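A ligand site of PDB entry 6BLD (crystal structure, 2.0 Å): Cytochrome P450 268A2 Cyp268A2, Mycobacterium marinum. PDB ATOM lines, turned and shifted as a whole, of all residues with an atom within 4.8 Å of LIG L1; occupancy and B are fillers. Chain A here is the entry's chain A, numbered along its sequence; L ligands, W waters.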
ATOM      1  N   SER A  74      16.515 -34.965  20.889  1.00  0.00           N
ATOM      2  CA  SER A  74      17.884 -34.467  20.780  1.00  0.00           C
ATOM      3  C   SER A  74      18.609 -35.034  19.569  1.00  0.00           C
ATOM      4  O   SER A  74      19.320 -34.314  18.864  1.00  0.00           O
ATOM      5  CB  SER A  74      18.662 -34.779  22.062  1.00  0.00           C
ATOM      6  OG  SER A  74      17.917 -34.429  23.203  1.00  0.00           O
ATOM      7  N   PHE A 102      26.509 -20.945  18.057  1.00  0.00           N
ATOM      8  CA  PHE A 102      26.087 -22.152  17.361  1.00  0.00           C
ATOM      9  C   PHE A 102      25.226 -23.074  18.212  1.00  0.00           C
ATOM     10  O   PHE A 102      24.779 -24.113  17.713  1.00  0.00           O
ATOM     11  CB  PHE A 102      27.306 -22.923  16.830  1.00  0.00           C
ATOM     12  CG  PHE A 102      28.269 -23.364  17.895  1.00  0.00           C
ATOM     13  CD1 PHE A 102      28.045 -24.504  18.642  1.00  0.00           C
ATOM     14  CD2 PHE A 102      29.436 -22.644  18.125  1.00  0.00           C
ATOM     15  CE1 PHE A 102      28.935 -24.909  19.613  1.00  0.00           C
ATOM     16  CE2 PHE A 102      30.338 -23.055  19.093  1.00  0.00           C
ATOM     17  CZ  PHE A 102      30.080 -24.182  19.843  1.00  0.00           C
ATOM     18  N   LEU A 103      24.969 -22.726  19.477  1.00  0.00           N
ATOM     19  CA  LEU A 103      24.011 -23.495  20.261  1.00  0.00           C
ATOM     20  C   LEU A 103      22.625 -23.447  19.631  1.00  0.00           C
ATOM     21  O   LEU A 103      21.930 -24.473  19.565  1.00  0.00           O
ATOM     22  CB  LEU A 103      23.974 -22.981  21.702  1.00  0.00           C
ATOM     23  CG  LEU A 103      22.913 -23.616  22.608  1.00  0.00           C
ATOM     24  CD1 LEU A 103      23.329 -25.019  23.028  1.00  0.00           C
ATOM     25  CD2 LEU A 103      22.670 -22.740  23.835  1.00  0.00           C
ATOM     26  N   HIS A 110      26.224 -24.783  12.050  1.00  0.00           N
ATOM     27  CA  HIS A 110      26.641 -25.306  13.341  1.00  0.00           C
ATOM     28  C   HIS A 110      27.874 -26.180  13.215  1.00  0.00           C
ATOM     29  O   HIS A 110      28.777 -26.131  14.070  1.00  0.00           O
ATOM     30  CB  HIS A 110      25.501 -26.090  13.993  1.00  0.00           C
ATOM     31  CG  HIS A 110      25.938 -26.917  15.163  1.00  0.00           C
ATOM     32  ND1 HIS A 110      26.349 -28.226  15.047  1.00  0.00           N
ATOM     33  CD2 HIS A 110      26.054 -26.615  16.479  1.00  0.00           C
ATOM     34  CE1 HIS A 110      26.691 -28.695  16.232  1.00  0.00           C
ATOM     35  NE2 HIS A 110      26.508 -27.738  17.126  1.00  0.00           N
ATOM     36  N   ARG A 114      31.315 -25.021  15.271  1.00  0.00           N
ATOM     37  CA  ARG A 114      31.763 -25.930  16.334  1.00  0.00           C
ATOM     38  C   ARG A 114      33.135 -26.521  16.005  1.00  0.00           C
ATOM     39  O   ARG A 114      33.948 -26.726  16.900  1.00  0.00           O
ATOM     40  CB  ARG A 114      30.728 -27.031  16.553  1.00  0.00           C
ATOM     41  CG  ARG A 114      31.217 -28.172  17.443  1.00  0.00           C
ATOM     42  CD  ARG A 114      30.071 -28.792  18.252  1.00  0.00           C
ATOM     43  NE  ARG A 114      30.539 -29.924  19.051  1.00  0.00           N
ATOM     44  CZ  ARG A 114      29.839 -30.481  20.036  1.00  0.00           C
ATOM     45  NH1 ARG A 114      28.630 -30.027  20.348  1.00  0.00           N
ATOM     46  NH2 ARG A 114      30.348 -31.507  20.705  1.00  0.00           N
ATOM     47  N   PHE A 121      38.673 -29.524  23.265  1.00  0.00           N
ATOM     48  CA  PHE A 121      37.817 -30.217  24.222  1.00  0.00           C
ATOM     49  C   PHE A 121      37.914 -31.731  24.157  1.00  0.00           C
ATOM     50  O   PHE A 121      37.227 -32.411  24.910  1.00  0.00           O
ATOM     51  CB  PHE A 121      36.355 -29.794  23.999  1.00  0.00           C
ATOM     52  CG  PHE A 121      36.076 -28.365  24.347  1.00  0.00           C
ATOM     53  CD1 PHE A 121      35.877 -27.990  25.657  1.00  0.00           C
ATOM     54  CD2 PHE A 121      36.014 -27.404  23.352  1.00  0.00           C
ATOM     55  CE1 PHE A 121      35.618 -26.673  25.986  1.00  0.00           C
ATOM     56  CE2 PHE A 121      35.759 -26.092  23.673  1.00  0.00           C
ATOM     57  CZ  PHE A 121      35.559 -25.717  24.983  1.00  0.00           C
ATOM     58  N   LEU A 256      28.449 -17.510  24.828  1.00  0.00           N
ATOM     59  CA  LEU A 256      28.079 -18.913  24.935  1.00  0.00           C
ATOM     60  C   LEU A 256      29.112 -19.697  25.747  1.00  0.00           C
ATOM     61  O   LEU A 256      28.750 -20.454  26.666  1.00  0.00           O
ATOM     62  CB  LEU A 256      27.924 -19.520  23.549  1.00  0.00           C
ATOM     63  CG  LEU A 256      27.768 -21.033  23.451  1.00  0.00           C
ATOM     64  CD1 LEU A 256      26.574 -21.525  24.269  1.00  0.00           C
ATOM     65  CD2 LEU A 256      27.678 -21.505  22.004  1.00  0.00           C
ATOM     66  N   LEU A 257      30.397 -19.497  25.456  1.00  0.00           N
ATOM     67  CA  LEU A 257      31.445 -20.224  26.159  1.00  0.00           C
ATOM     68  C   LEU A 257      31.523 -19.799  27.620  1.00  0.00           C
ATOM     69  O   LEU A 257      31.717 -20.649  28.509  1.00  0.00           O
ATOM     70  CB  LEU A 257      32.794 -20.001  25.472  1.00  0.00           C
ATOM     71  CG  LEU A 257      34.015 -20.760  25.979  1.00  0.00           C
ATOM     72  CD1 LEU A 257      33.720 -22.241  26.055  1.00  0.00           C
ATOM     73  CD2 LEU A 257      35.169 -20.493  25.038  1.00  0.00           C
ATOM     74  N   ALA A 260      28.024 -21.252  29.418  1.00  0.00           N
ATOM     75  CA  ALA A 260      28.001 -22.700  29.538  1.00  0.00           C
ATOM     76  C   ALA A 260      29.224 -23.229  30.289  1.00  0.00           C
ATOM     77  O   ALA A 260      29.109 -24.224  31.026  1.00  0.00           O
ATOM     78  CB  ALA A 260      27.919 -23.342  28.156  1.00  0.00           C
ATOM     79  N   GLY A 261      30.372 -22.580  30.138  1.00  0.00           N
ATOM     80  CA  GLY A 261      31.572 -23.032  30.815  1.00  0.00           C
ATOM     81  C   GLY A 261      31.633 -22.700  32.291  1.00  0.00           C
ATOM     82  O   GLY A 261      32.365 -23.365  33.035  1.00  0.00           O
ATOM     83  N   THR A 264      27.168 -23.987  34.531  1.00  0.00           N
ATOM     84  CA  THR A 264      26.799 -25.393  34.704  1.00  0.00           C
ATOM     85  C   THR A 264      27.687 -26.084  35.736  1.00  0.00           C
ATOM     86  O   THR A 264      27.189 -26.706  36.685  1.00  0.00           O
ATOM     87  CB  THR A 264      26.889 -26.120  33.364  1.00  0.00           C
ATOM     88  OG1 THR A 264      28.207 -25.957  32.817  1.00  0.00           O
ATOM     89  CG2 THR A 264      25.872 -25.557  32.386  1.00  0.00           C
ATOM     90  N   THR A 265      29.012 -25.987  35.569  1.00  0.00           N
ATOM     91  CA  THR A 265      29.918 -26.625  36.509  1.00  0.00           C
ATOM     92  C   THR A 265      29.798 -26.022  37.907  1.00  0.00           C
ATOM     93  O   THR A 265      29.858 -26.744  38.908  1.00  0.00           O
ATOM     94  CB  THR A 265      31.356 -26.519  36.002  1.00  0.00           C
ATOM     95  OG1 THR A 265      31.420 -26.943  34.640  1.00  0.00           O
ATOM     96  CG2 THR A 265      32.300 -27.386  36.843  1.00  0.00           C
ATOM     97  N   THR A 268      26.809 -27.549  39.565  1.00  0.00           N
ATOM     98  CA  THR A 268      27.030 -28.960  39.857  1.00  0.00           C
ATOM     99  C   THR A 268      27.929 -29.145  41.081  1.00  0.00           C
ATOM    100  O   THR A 268      27.744 -30.086  41.854  1.00  0.00           O
ATOM    101  CB  THR A 268      27.635 -29.667  38.635  1.00  0.00           C
ATOM    102  OG1 THR A 268      26.802 -29.428  37.493  1.00  0.00           O
ATOM    103  CG2 THR A 268      27.727 -31.165  38.877  1.00  0.00           C
ATOM    104  N   VAL A 302      26.324 -35.248  38.324  1.00  0.00           N
ATOM    105  CA  VAL A 302      25.748 -34.493  37.218  1.00  0.00           C
ATOM    106  C   VAL A 302      24.265 -34.812  37.071  1.00  0.00           C
ATOM    107  O   VAL A 302      23.442 -33.917  36.875  1.00  0.00           O
ATOM    108  CB  VAL A 302      26.524 -34.772  35.916  1.00  0.00           C
ATOM    109  CG1 VAL A 302      25.748 -34.267  34.711  1.00  0.00           C
ATOM    110  CG2 VAL A 302      27.901 -34.169  35.970  1.00  0.00           C
ATOM    111  N   PRO A 307      22.138 -29.236  36.067  1.00  0.00           N
ATOM    112  CA  PRO A 307      22.142 -27.761  36.124  1.00  0.00           C
ATOM    113  C   PRO A 307      21.385 -27.117  34.975  1.00  0.00           C
ATOM    114  O   PRO A 307      20.832 -26.032  35.153  1.00  0.00           O
ATOM    115  CB  PRO A 307      23.642 -27.415  36.083  1.00  0.00           C
ATOM    116  CG  PRO A 307      24.276 -28.568  35.413  1.00  0.00           C
ATOM    117  CD  PRO A 307      23.487 -29.780  35.837  1.00  0.00           C
ATOM    118  N   VAL A 308      21.349 -27.756  33.815  1.00  0.00           N
ATOM    119  CA  VAL A 308      20.520 -27.300  32.709  1.00  0.00           C
ATOM    120  C   VAL A 308      19.196 -28.052  32.789  1.00  0.00           C
ATOM    121  O   VAL A 308      19.150 -29.264  32.552  1.00  0.00           O
ATOM    122  CB  VAL A 308      21.206 -27.516  31.351  1.00  0.00           C
ATOM    123  CG1 VAL A 308      20.362 -26.933  30.231  1.00  0.00           C
ATOM    124  CG2 VAL A 308      22.596 -26.908  31.357  1.00  0.00           C
ATOM    125  N   PHE A 311      15.860 -27.189  27.578  1.00  0.00           N
ATOM    126  CA  PHE A 311      16.277 -26.724  26.265  1.00  0.00           C
ATOM    127  C   PHE A 311      15.158 -27.103  25.306  1.00  0.00           C
ATOM    128  O   PHE A 311      14.501 -28.123  25.482  1.00  0.00           O
ATOM    129  CB  PHE A 311      17.611 -27.320  25.808  1.00  0.00           C
ATOM    130  CG  PHE A 311      18.809 -26.453  26.094  1.00  0.00           C
ATOM    131  CD1 PHE A 311      18.745 -25.079  25.908  1.00  0.00           C
ATOM    132  CD2 PHE A 311      19.985 -27.010  26.550  1.00  0.00           C
ATOM    133  CE1 PHE A 311      19.845 -24.282  26.174  1.00  0.00           C
ATOM    134  CE2 PHE A 311      21.094 -26.215  26.821  1.00  0.00           C
ATOM    135  CZ  PHE A 311      21.021 -24.853  26.626  1.00  0.00           C
ATOM    136  N   ARG A 313      13.360 -27.104  21.140  1.00  0.00           N
ATOM    137  CA  ARG A 313      13.573 -27.251  19.710  1.00  0.00           C
ATOM    138  C   ARG A 313      12.324 -26.786  18.978  1.00  0.00           C
ATOM    139  O   ARG A 313      11.267 -26.586  19.587  1.00  0.00           O
ATOM    140  CB  ARG A 313      13.915 -28.697  19.324  1.00  0.00           C
ATOM    141  CG  ARG A 313      15.125 -29.284  20.044  1.00  0.00           C
ATOM    142  CD  ARG A 313      16.423 -28.787  19.446  1.00  0.00           C
ATOM    143  NE  ARG A 313      17.592 -29.517  19.950  1.00  0.00           N
ATOM    144  CZ  ARG A 313      18.341 -29.111  20.960  1.00  0.00           C
ATOM    145  NH1 ARG A 313      18.049 -27.981  21.590  1.00  0.00           N
ATOM    146  NH2 ARG A 313      19.387 -29.831  21.353  1.00  0.00           N
ATOM    147  N   TYR A 336      15.076 -31.855  31.286  1.00  0.00           N
ATOM    148  CA  TYR A 336      16.136 -32.780  31.656  1.00  0.00           C
ATOM    149  C   TYR A 336      16.002 -33.283  33.091  1.00  0.00           C
ATOM    150  O   TYR A 336      16.360 -34.422  33.387  1.00  0.00           O
ATOM    151  CB  TYR A 336      17.502 -32.118  31.450  1.00  0.00           C
ATOM    152  CG  TYR A 336      17.753 -31.642  30.044  1.00  0.00           C
ATOM    153  CD1 TYR A 336      18.036 -30.311  29.782  1.00  0.00           C
ATOM    154  CD2 TYR A 336      17.704 -32.524  28.975  1.00  0.00           C
ATOM    155  CE1 TYR A 336      18.272 -29.864  28.491  1.00  0.00           C
ATOM    156  CE2 TYR A 336      17.940 -32.091  27.682  1.00  0.00           C
ATOM    157  CZ  TYR A 336      18.228 -30.768  27.452  1.00  0.00           C
ATOM    158  OH  TYR A 336      18.462 -30.343  26.163  1.00  0.00           O
ATOM    159  N   GLY A 363      22.047 -35.154  31.674  1.00  0.00           N
ATOM    160  CA  GLY A 363      22.561 -33.905  32.216  1.00  0.00           C
ATOM    161  C   GLY A 363      23.300 -33.079  31.185  1.00  0.00           C
ATOM    162  O   GLY A 363      23.223 -31.845  31.176  1.00  0.00           O
ATOM    163  N   PHE A 364      24.028 -33.747  30.285  1.00  0.00           N
ATOM    164  CA  PHE A 364      24.665 -33.103  29.151  1.00  0.00           C
ATOM    165  C   PHE A 364      23.764 -33.085  27.922  1.00  0.00           C
ATOM    166  O   PHE A 364      24.266 -32.938  26.804  1.00  0.00           O
ATOM    167  CB  PHE A 364      25.994 -33.798  28.821  1.00  0.00           C
ATOM    168  CG  PHE A 364      27.021 -33.682  29.914  1.00  0.00           C
ATOM    169  CD1 PHE A 364      27.597 -32.462  30.234  1.00  0.00           C
ATOM    170  CD2 PHE A 364      27.437 -34.813  30.613  1.00  0.00           C
ATOM    171  CE1 PHE A 364      28.546 -32.368  31.232  1.00  0.00           C
ATOM    172  CE2 PHE A 364      28.386 -34.719  31.610  1.00  0.00           C
ATOM    173  CZ  PHE A 364      28.945 -33.497  31.922  1.00  0.00           C
ATOM    174  N   GLY A 365      22.457 -33.223  28.112  1.00  0.00           N
ATOM    175  CA  GLY A 365      21.518 -33.290  27.012  1.00  0.00           C
ATOM    176  C   GLY A 365      21.226 -34.718  26.595  1.00  0.00           C
ATOM    177  O   GLY A 365      21.809 -35.687  27.081  1.00  0.00           O
ATOM    178  N   GLY A 366      20.288 -34.842  25.661  1.00  0.00           N
ATOM    179  CA  GLY A 366      19.903 -36.150  25.162  1.00  0.00           C
ATOM    180  C   GLY A 366      20.842 -36.765  24.165  1.00  0.00           C
ATOM    181  O   GLY A 366      20.568 -37.852  23.645  1.00  0.00           O
ATOM    182  N   GLY A 367      21.970 -36.110  23.874  1.00  0.00           N
ATOM    183  CA  GLY A 367      22.933 -36.619  22.918  1.00  0.00           C
ATOM    184  C   GLY A 367      22.639 -36.170  21.499  1.00  0.00           C
ATOM    185  O   GLY A 367      21.551 -35.713  21.161  1.00  0.00           O
ATOM    186  N   VAL A 369      23.836 -34.025  17.906  1.00  0.00           N
ATOM    187  CA  VAL A 369      24.622 -33.003  17.224  1.00  0.00           C
ATOM    188  C   VAL A 369      25.111 -31.941  18.210  1.00  0.00           C
ATOM    189  O   VAL A 369      26.257 -31.475  18.115  1.00  0.00           O
ATOM    190  CB  VAL A 369      23.790 -32.385  16.086  1.00  0.00           C
ATOM    191  CG1 VAL A 369      24.306 -31.023  15.699  1.00  0.00           C
ATOM    192  CG2 VAL A 369      23.799 -33.315  14.870  1.00  0.00           C
ATOM    193  N   HIS A 370      24.280 -31.547  19.171  1.00  0.00           N
ATOM    194  CA  HIS A 370      24.605 -30.464  20.085  1.00  0.00           C
ATOM    195  C   HIS A 370      25.131 -30.961  21.432  1.00  0.00           C
ATOM    196  O   HIS A 370      25.120 -30.194  22.398  1.00  0.00           O
ATOM    197  CB  HIS A 370      23.375 -29.583  20.297  1.00  0.00           C
ATOM    198  CG  HIS A 370      23.067 -28.695  19.129  1.00  0.00           C
ATOM    199  ND1 HIS A 370      23.579 -27.421  19.004  1.00  0.00           N
ATOM    200  CD2 HIS A 370      22.299 -28.898  18.040  1.00  0.00           C
ATOM    201  CE1 HIS A 370      23.131 -26.879  17.891  1.00  0.00           C
ATOM    202  NE2 HIS A 370      22.361 -27.754  17.283  1.00  0.00           N
ATOM    203  N   PHE A 371      25.589 -32.201  21.508  1.00  0.00           N
ATOM    204  CA  PHE A 371      26.047 -32.761  22.778  1.00  0.00           C
ATOM    205  C   PHE A 371      27.143 -31.884  23.383  1.00  0.00           C
ATOM    206  O   PHE A 371      27.983 -31.324  22.661  1.00  0.00           O
ATOM    207  CB  PHE A 371      26.565 -34.184  22.605  1.00  0.00           C
ATOM    208  CG  PHE A 371      26.919 -34.857  23.904  1.00  0.00           C
ATOM    209  CD1 PHE A 371      25.929 -35.405  24.707  1.00  0.00           C
ATOM    210  CD2 PHE A 371      28.234 -34.935  24.333  1.00  0.00           C
ATOM    211  CE1 PHE A 371      26.240 -36.022  25.901  1.00  0.00           C
ATOM    212  CE2 PHE A 371      28.554 -35.554  25.531  1.00  0.00           C
ATOM    213  CZ  PHE A 371      27.549 -36.092  26.320  1.00  0.00           C
ATOM    214  N   CYS A 372      27.134 -31.792  24.708  1.00  0.00           N
ATOM    215  CA  CYS A 372      27.909 -30.796  25.441  1.00  0.00           C
ATOM    216  C   CYS A 372      29.360 -30.788  25.004  1.00  0.00           C
ATOM    217  O   CYS A 372      30.057 -31.798  25.094  1.00  0.00           O
ATOM    218  CB  CYS A 372      27.814 -31.057  26.937  1.00  0.00           C
ATOM    219  SG  CYS A 372      29.111 -30.249  27.892  1.00  0.00           S
ATOM    220  N   LEU A 373      29.819 -29.625  24.533  1.00  0.00           N
ATOM    221  CA  LEU A 373      31.196 -29.501  24.064  1.00  0.00           C
ATOM    222  C   LEU A 373      32.206 -29.661  25.205  1.00  0.00           C
ATOM    223  O   LEU A 373      33.307 -30.159  24.965  1.00  0.00           O
ATOM    224  CB  LEU A 373      31.368 -28.136  23.400  1.00  0.00           C
ATOM    225  CG  LEU A 373      32.634 -27.822  22.604  1.00  0.00           C
ATOM    226  CD1 LEU A 373      33.180 -29.045  21.852  1.00  0.00           C
ATOM    227  CD2 LEU A 373      32.424 -26.644  21.657  1.00  0.00           C
ATOM    228  N   GLY A 374      31.852 -29.241  26.406  1.00  0.00           N
ATOM    229  CA  GLY A 374      32.810 -29.294  27.492  1.00  0.00           C
ATOM    230  C   GLY A 374      32.581 -30.429  28.476  1.00  0.00           C
ATOM    231  O   GLY A 374      32.913 -30.306  29.659  1.00  0.00           O
ATOM    232  N   LEU A 377      35.821 -31.715  29.821  1.00  0.00           N
ATOM    233  CA  LEU A 377      36.396 -30.682  30.673  1.00  0.00           C
ATOM    234  C   LEU A 377      35.626 -30.557  31.978  1.00  0.00           C
ATOM    235  O   LEU A 377      36.224 -30.388  33.042  1.00  0.00           O
ATOM    236  CB  LEU A 377      36.406 -29.351  29.923  1.00  0.00           C
ATOM    237  CG  LEU A 377      36.983 -28.150  30.689  1.00  0.00           C
ATOM    238  CD1 LEU A 377      38.504 -28.232  30.724  1.00  0.00           C
ATOM    239  CD2 LEU A 377      36.531 -26.847  30.051  1.00  0.00           C
ATOM    240  N   ALA A 378      34.293 -30.624  31.919  1.00  0.00           N
ATOM    241  CA  ALA A 378      33.493 -30.557  33.136  1.00  0.00           C
ATOM    242  C   ALA A 378      33.812 -31.722  34.070  1.00  0.00           C
ATOM    243  O   ALA A 378      33.985 -31.521  35.274  1.00  0.00           O
ATOM    244  CB  ALA A 378      32.008 -30.542  32.790  1.00  0.00           C
ATOM    245  N   GLN A 381      36.982 -31.225  35.887  1.00  0.00           N
ATOM    246  CA  GLN A 381      36.872 -30.239  36.959  1.00  0.00           C
ATOM    247  C   GLN A 381      36.209 -30.832  38.199  1.00  0.00           C
ATOM    248  O   GLN A 381      36.652 -30.566  39.324  1.00  0.00           O
ATOM    249  CB  GLN A 381      36.079 -29.021  36.472  1.00  0.00           C
ATOM    250  CG  GLN A 381      36.806 -28.204  35.416  1.00  0.00           C
ATOM    251  CD  GLN A 381      36.072 -26.909  35.096  1.00  0.00           C
ATOM    252  OE1 GLN A 381      35.737 -26.147  35.989  1.00  0.00           O
ATOM    253  NE2 GLN A 381      35.838 -26.674  33.806  1.00  0.00           N
HETATM  254  C1  LIG L   1      26.021 -27.700  25.227  1.00  0.00           C
HETATM  255  C2  LIG L   1      30.214 -25.716  26.653  1.00  0.00           C
HETATM  256  C3  LIG L   1      29.774 -27.872  30.976  1.00  0.00           C
HETATM  257  C4  LIG L   1      25.216 -29.092  29.804  1.00  0.00           C
HETATM  258  C5  LIG L   1      27.198 -26.981  25.233  1.00  0.00           C
HETATM  259  C6  LIG L   1      27.735 -26.207  24.124  1.00  0.00           C
HETATM  260  C7  LIG L   1      28.884 -25.660  24.512  1.00  0.00           C
HETATM  261  C8  LIG L   1      29.137 -26.070  25.887  1.00  0.00           C
HETATM  262  C9  LIG L   1      29.799 -24.758  23.659  1.00  0.00           C
HETATM  263  C10 LIG L   1      27.080 -26.048  22.741  1.00  0.00           C
HETATM  264  C11 LIG L   1      27.442 -27.258  21.888  1.00  0.00           C
HETATM  265  C12 LIG L   1      26.672 -27.235  20.598  1.00  0.00           C
HETATM  266  O1  LIG L   1      27.081 -27.940  19.635  1.00  0.00           O
HETATM  267  O2  LIG L   1      25.652 -26.506  20.516  1.00  0.00           O
HETATM  268  C13 LIG L   1      30.501 -26.179  27.925  1.00  0.00           C
HETATM  269  C14 LIG L   1      31.738 -25.981  28.633  1.00  0.00           C
HETATM  270  C15 LIG L   1      31.650 -26.566  29.824  1.00  0.00           C
HETATM  271  C16 LIG L   1      30.320 -27.164  29.926  1.00  0.00           C
HETATM  272  C17 LIG L   1      32.980 -25.226  28.109  1.00  0.00           C
HETATM  273  C18 LIG L   1      32.798 -26.548  30.856  1.00  0.00           C
HETATM  274  C19 LIG L   1      32.756 -27.230  32.003  1.00  0.00           C
HETATM  275  C20 LIG L   1      28.500 -28.401  31.044  1.00  0.00           C
HETATM  276  C21 LIG L   1      27.927 -29.158  32.140  1.00  0.00           C
HETATM  277  C22 LIG L   1      26.660 -29.482  31.807  1.00  0.00           C
HETATM  278  C23 LIG L   1      26.403 -28.948  30.489  1.00  0.00           C
HETATM  279  C24 LIG L   1      28.693 -29.477  33.447  1.00  0.00           C
HETATM  280  C25 LIG L   1      25.601 -30.289  32.586  1.00  0.00           C
HETATM  281  C26 LIG L   1      25.859 -30.994  33.687  1.00  0.00           C
HETATM  282  C27 LIG L   1      25.032 -28.842  28.463  1.00  0.00           C
HETATM  283  C28 LIG L   1      23.826 -29.113  27.701  1.00  0.00           C
HETATM  284  C29 LIG L   1      24.044 -28.731  26.433  1.00  0.00           C
HETATM  285  C30 LIG L   1      25.403 -28.203  26.351  1.00  0.00           C
HETATM  286  C31 LIG L   1      22.531 -29.734  28.267  1.00  0.00           C
HETATM  287  C32 LIG L   1      23.044 -28.834  25.267  1.00  0.00           C
HETATM  288  C33 LIG L   1      23.027 -30.271  24.746  1.00  0.00           C
HETATM  289  C34 LIG L   1      22.015 -30.434  23.639  1.00  0.00           C
HETATM  290  O3  LIG L   1      21.852 -31.578  23.153  1.00  0.00           O
HETATM  291  O4  LIG L   1      21.388 -29.425  23.248  1.00  0.00           O
HETATM  292  N1  LIG L   1      28.087 -26.874  26.285  1.00  0.00           N
HETATM  293  N2  LIG L   1      29.660 -26.907  28.732  1.00  0.00           N
HETATM  294  N3  LIG L   1      27.536 -28.299  30.050  1.00  0.00           N
HETATM  295  N4  LIG L   1      25.957 -28.283  27.612  1.00  0.00           N
HETATM  296 FE1  LIG L   1      27.889 -27.805  28.104  1.00  0.00          FE
HETATM  297  C1  LG2 L   2      22.200 -16.934  27.461  1.00  0.00           C
HETATM  298  C2  LG2 L   2      19.900 -14.062  28.530  1.00  0.00           C
HETATM  299  C3  LG2 L   2      24.491 -25.173  28.017  1.00  0.00           C
HETATM  300  C4  LG2 L   2      24.271 -23.706  28.366  1.00  0.00           C
HETATM  301  C5  LG2 L   2      24.347 -22.791  27.423  1.00  0.00           C
HETATM  302  C6  LG2 L   2      23.973 -23.297  29.814  1.00  0.00           C
HETATM  303  C7  LG2 L   2      24.143 -21.309  27.742  1.00  0.00           C
HETATM  304  C8  LG2 L   2      23.169 -20.642  26.765  1.00  0.00           C
HETATM  305  C9  LG2 L   2      23.198 -19.115  26.850  1.00  0.00           C
HETATM  306  C10 LG2 L   2      22.183 -18.467  27.373  1.00  0.00           C
HETATM  307  C11 LG2 L   2      24.415 -18.348  26.332  1.00  0.00           C
HETATM  308  C12 LG2 L   2      21.079 -16.288  27.747  1.00  0.00           C
HETATM  309  C13 LG2 L   2      21.072 -14.770  27.835  1.00  0.00           C
HETATM  310  O1  LG2 L   2      21.955 -14.138  27.377  1.00  0.00           O
HETATM  311  O   HOH W   1      19.471 -32.307  24.419  1.00  0.00           O
HETATM  312  O   HOH W   2      20.167 -27.045  23.197  1.00  0.00           O
HETATM  313  O   HOH W   3      22.159 -32.670  20.581  1.00  0.00           O
HETATM  314  O   HOH W   4      23.190 -33.692  24.264  1.00  0.00           O
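The side-chain sulfur (SG) of Cys 372 binds an iron atom (FE1) of LIG L1 (2.7 Å). A ring nitrogen (NE2) of His 110 lies within hydrogen-bond range of an oxygen (O1) of LIG L1, at 2.6 Å. An oxygen (O4) of LIG L1 is in salt-bridge range of the guanidinium group (NH2) of Arg 313 (2.8 Å). A ring nitrogen (ND1) of His 370 lies within hydrogen-bond range of an oxygen (O2) of LIG L1. An oxygen (O1) of LIG L1 is in salt-bridge range of the guanidinium group of Arg 114 (2.7 Å).
The side-chain hydroxyl of Thr 264 is in hydrogen-bond range of the backbone carbonyl oxygen of Ala 260. NE2 of His 110 is in hydrogen-bond range of ND1 of His 370, 3.5 Å away. The backbone carbonyl oxygen (O) of Leu 103 lies close to a ring nitrogen (ND1) of His 370 (3.4 Å). SG of Cys 372 sits close to N of Gly 374 (3.3 Å). O of Thr 264 lies within hydrogen-bond range of OG1 of Thr 268, 2.9 Å away. The guanidinium group (NH1) of Arg 114 lies within hydrogen-bond range of the backbone carbonyl oxygen (O) of Phe 371 (2.7 Å).
Water W2 bridges O4 of LIG L1 (2.7 Å) and NH1 of Arg 313 (2.8 Å). Water W4 lies within hydrogen-bond range of the backbone NH of Gly 367 (2.7 Å), an oxygen (O3) of LIG L1 (2.7 Å), the backbone carbonyl oxygen of Phe 364 (2.9 Å) and the backbone NH of Gly 366 (3.4 Å). Water W1 lies within hydrogen-bond range of O3 of LIG L1, OH of Tyr 336, OG of Ser 74 and N of Gly 366. Water W3 lies within hydrogen-bond range of N of His 370 (2.8 Å), O3 of LIG L1 (2.8 Å), O of Gly 367 (3.2 Å) and N of Val 369 (3.4 Å).
Merely in contact with LIG L1: Thr 265 (3.0 Å), Thr 264 (3.0 Å), Gly 363 (3.2 Å), Ala 260 (3.4 Å), Pro 307 (3.4 Å), Phe 102 (3.4 Å), Phe 364 (3.4 Å), Val 302 (3.4 Å), Leu 103 (3.4 Å), Ala 378 (3.5 Å), Gly 365 (3.5 Å), Gln 381 (3.6 Å), Phe 311 (3.6 Å), Gly 374 (3.7 Å), Gly 261 (3.7 Å), Leu 373 (3.7 Å), Phe 121 (3.7 Å), Leu 257 (3.7 Å), Val 308 (3.7 Å), Leu 377 (3.8 Å) and Val 369 (3.9 Å).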
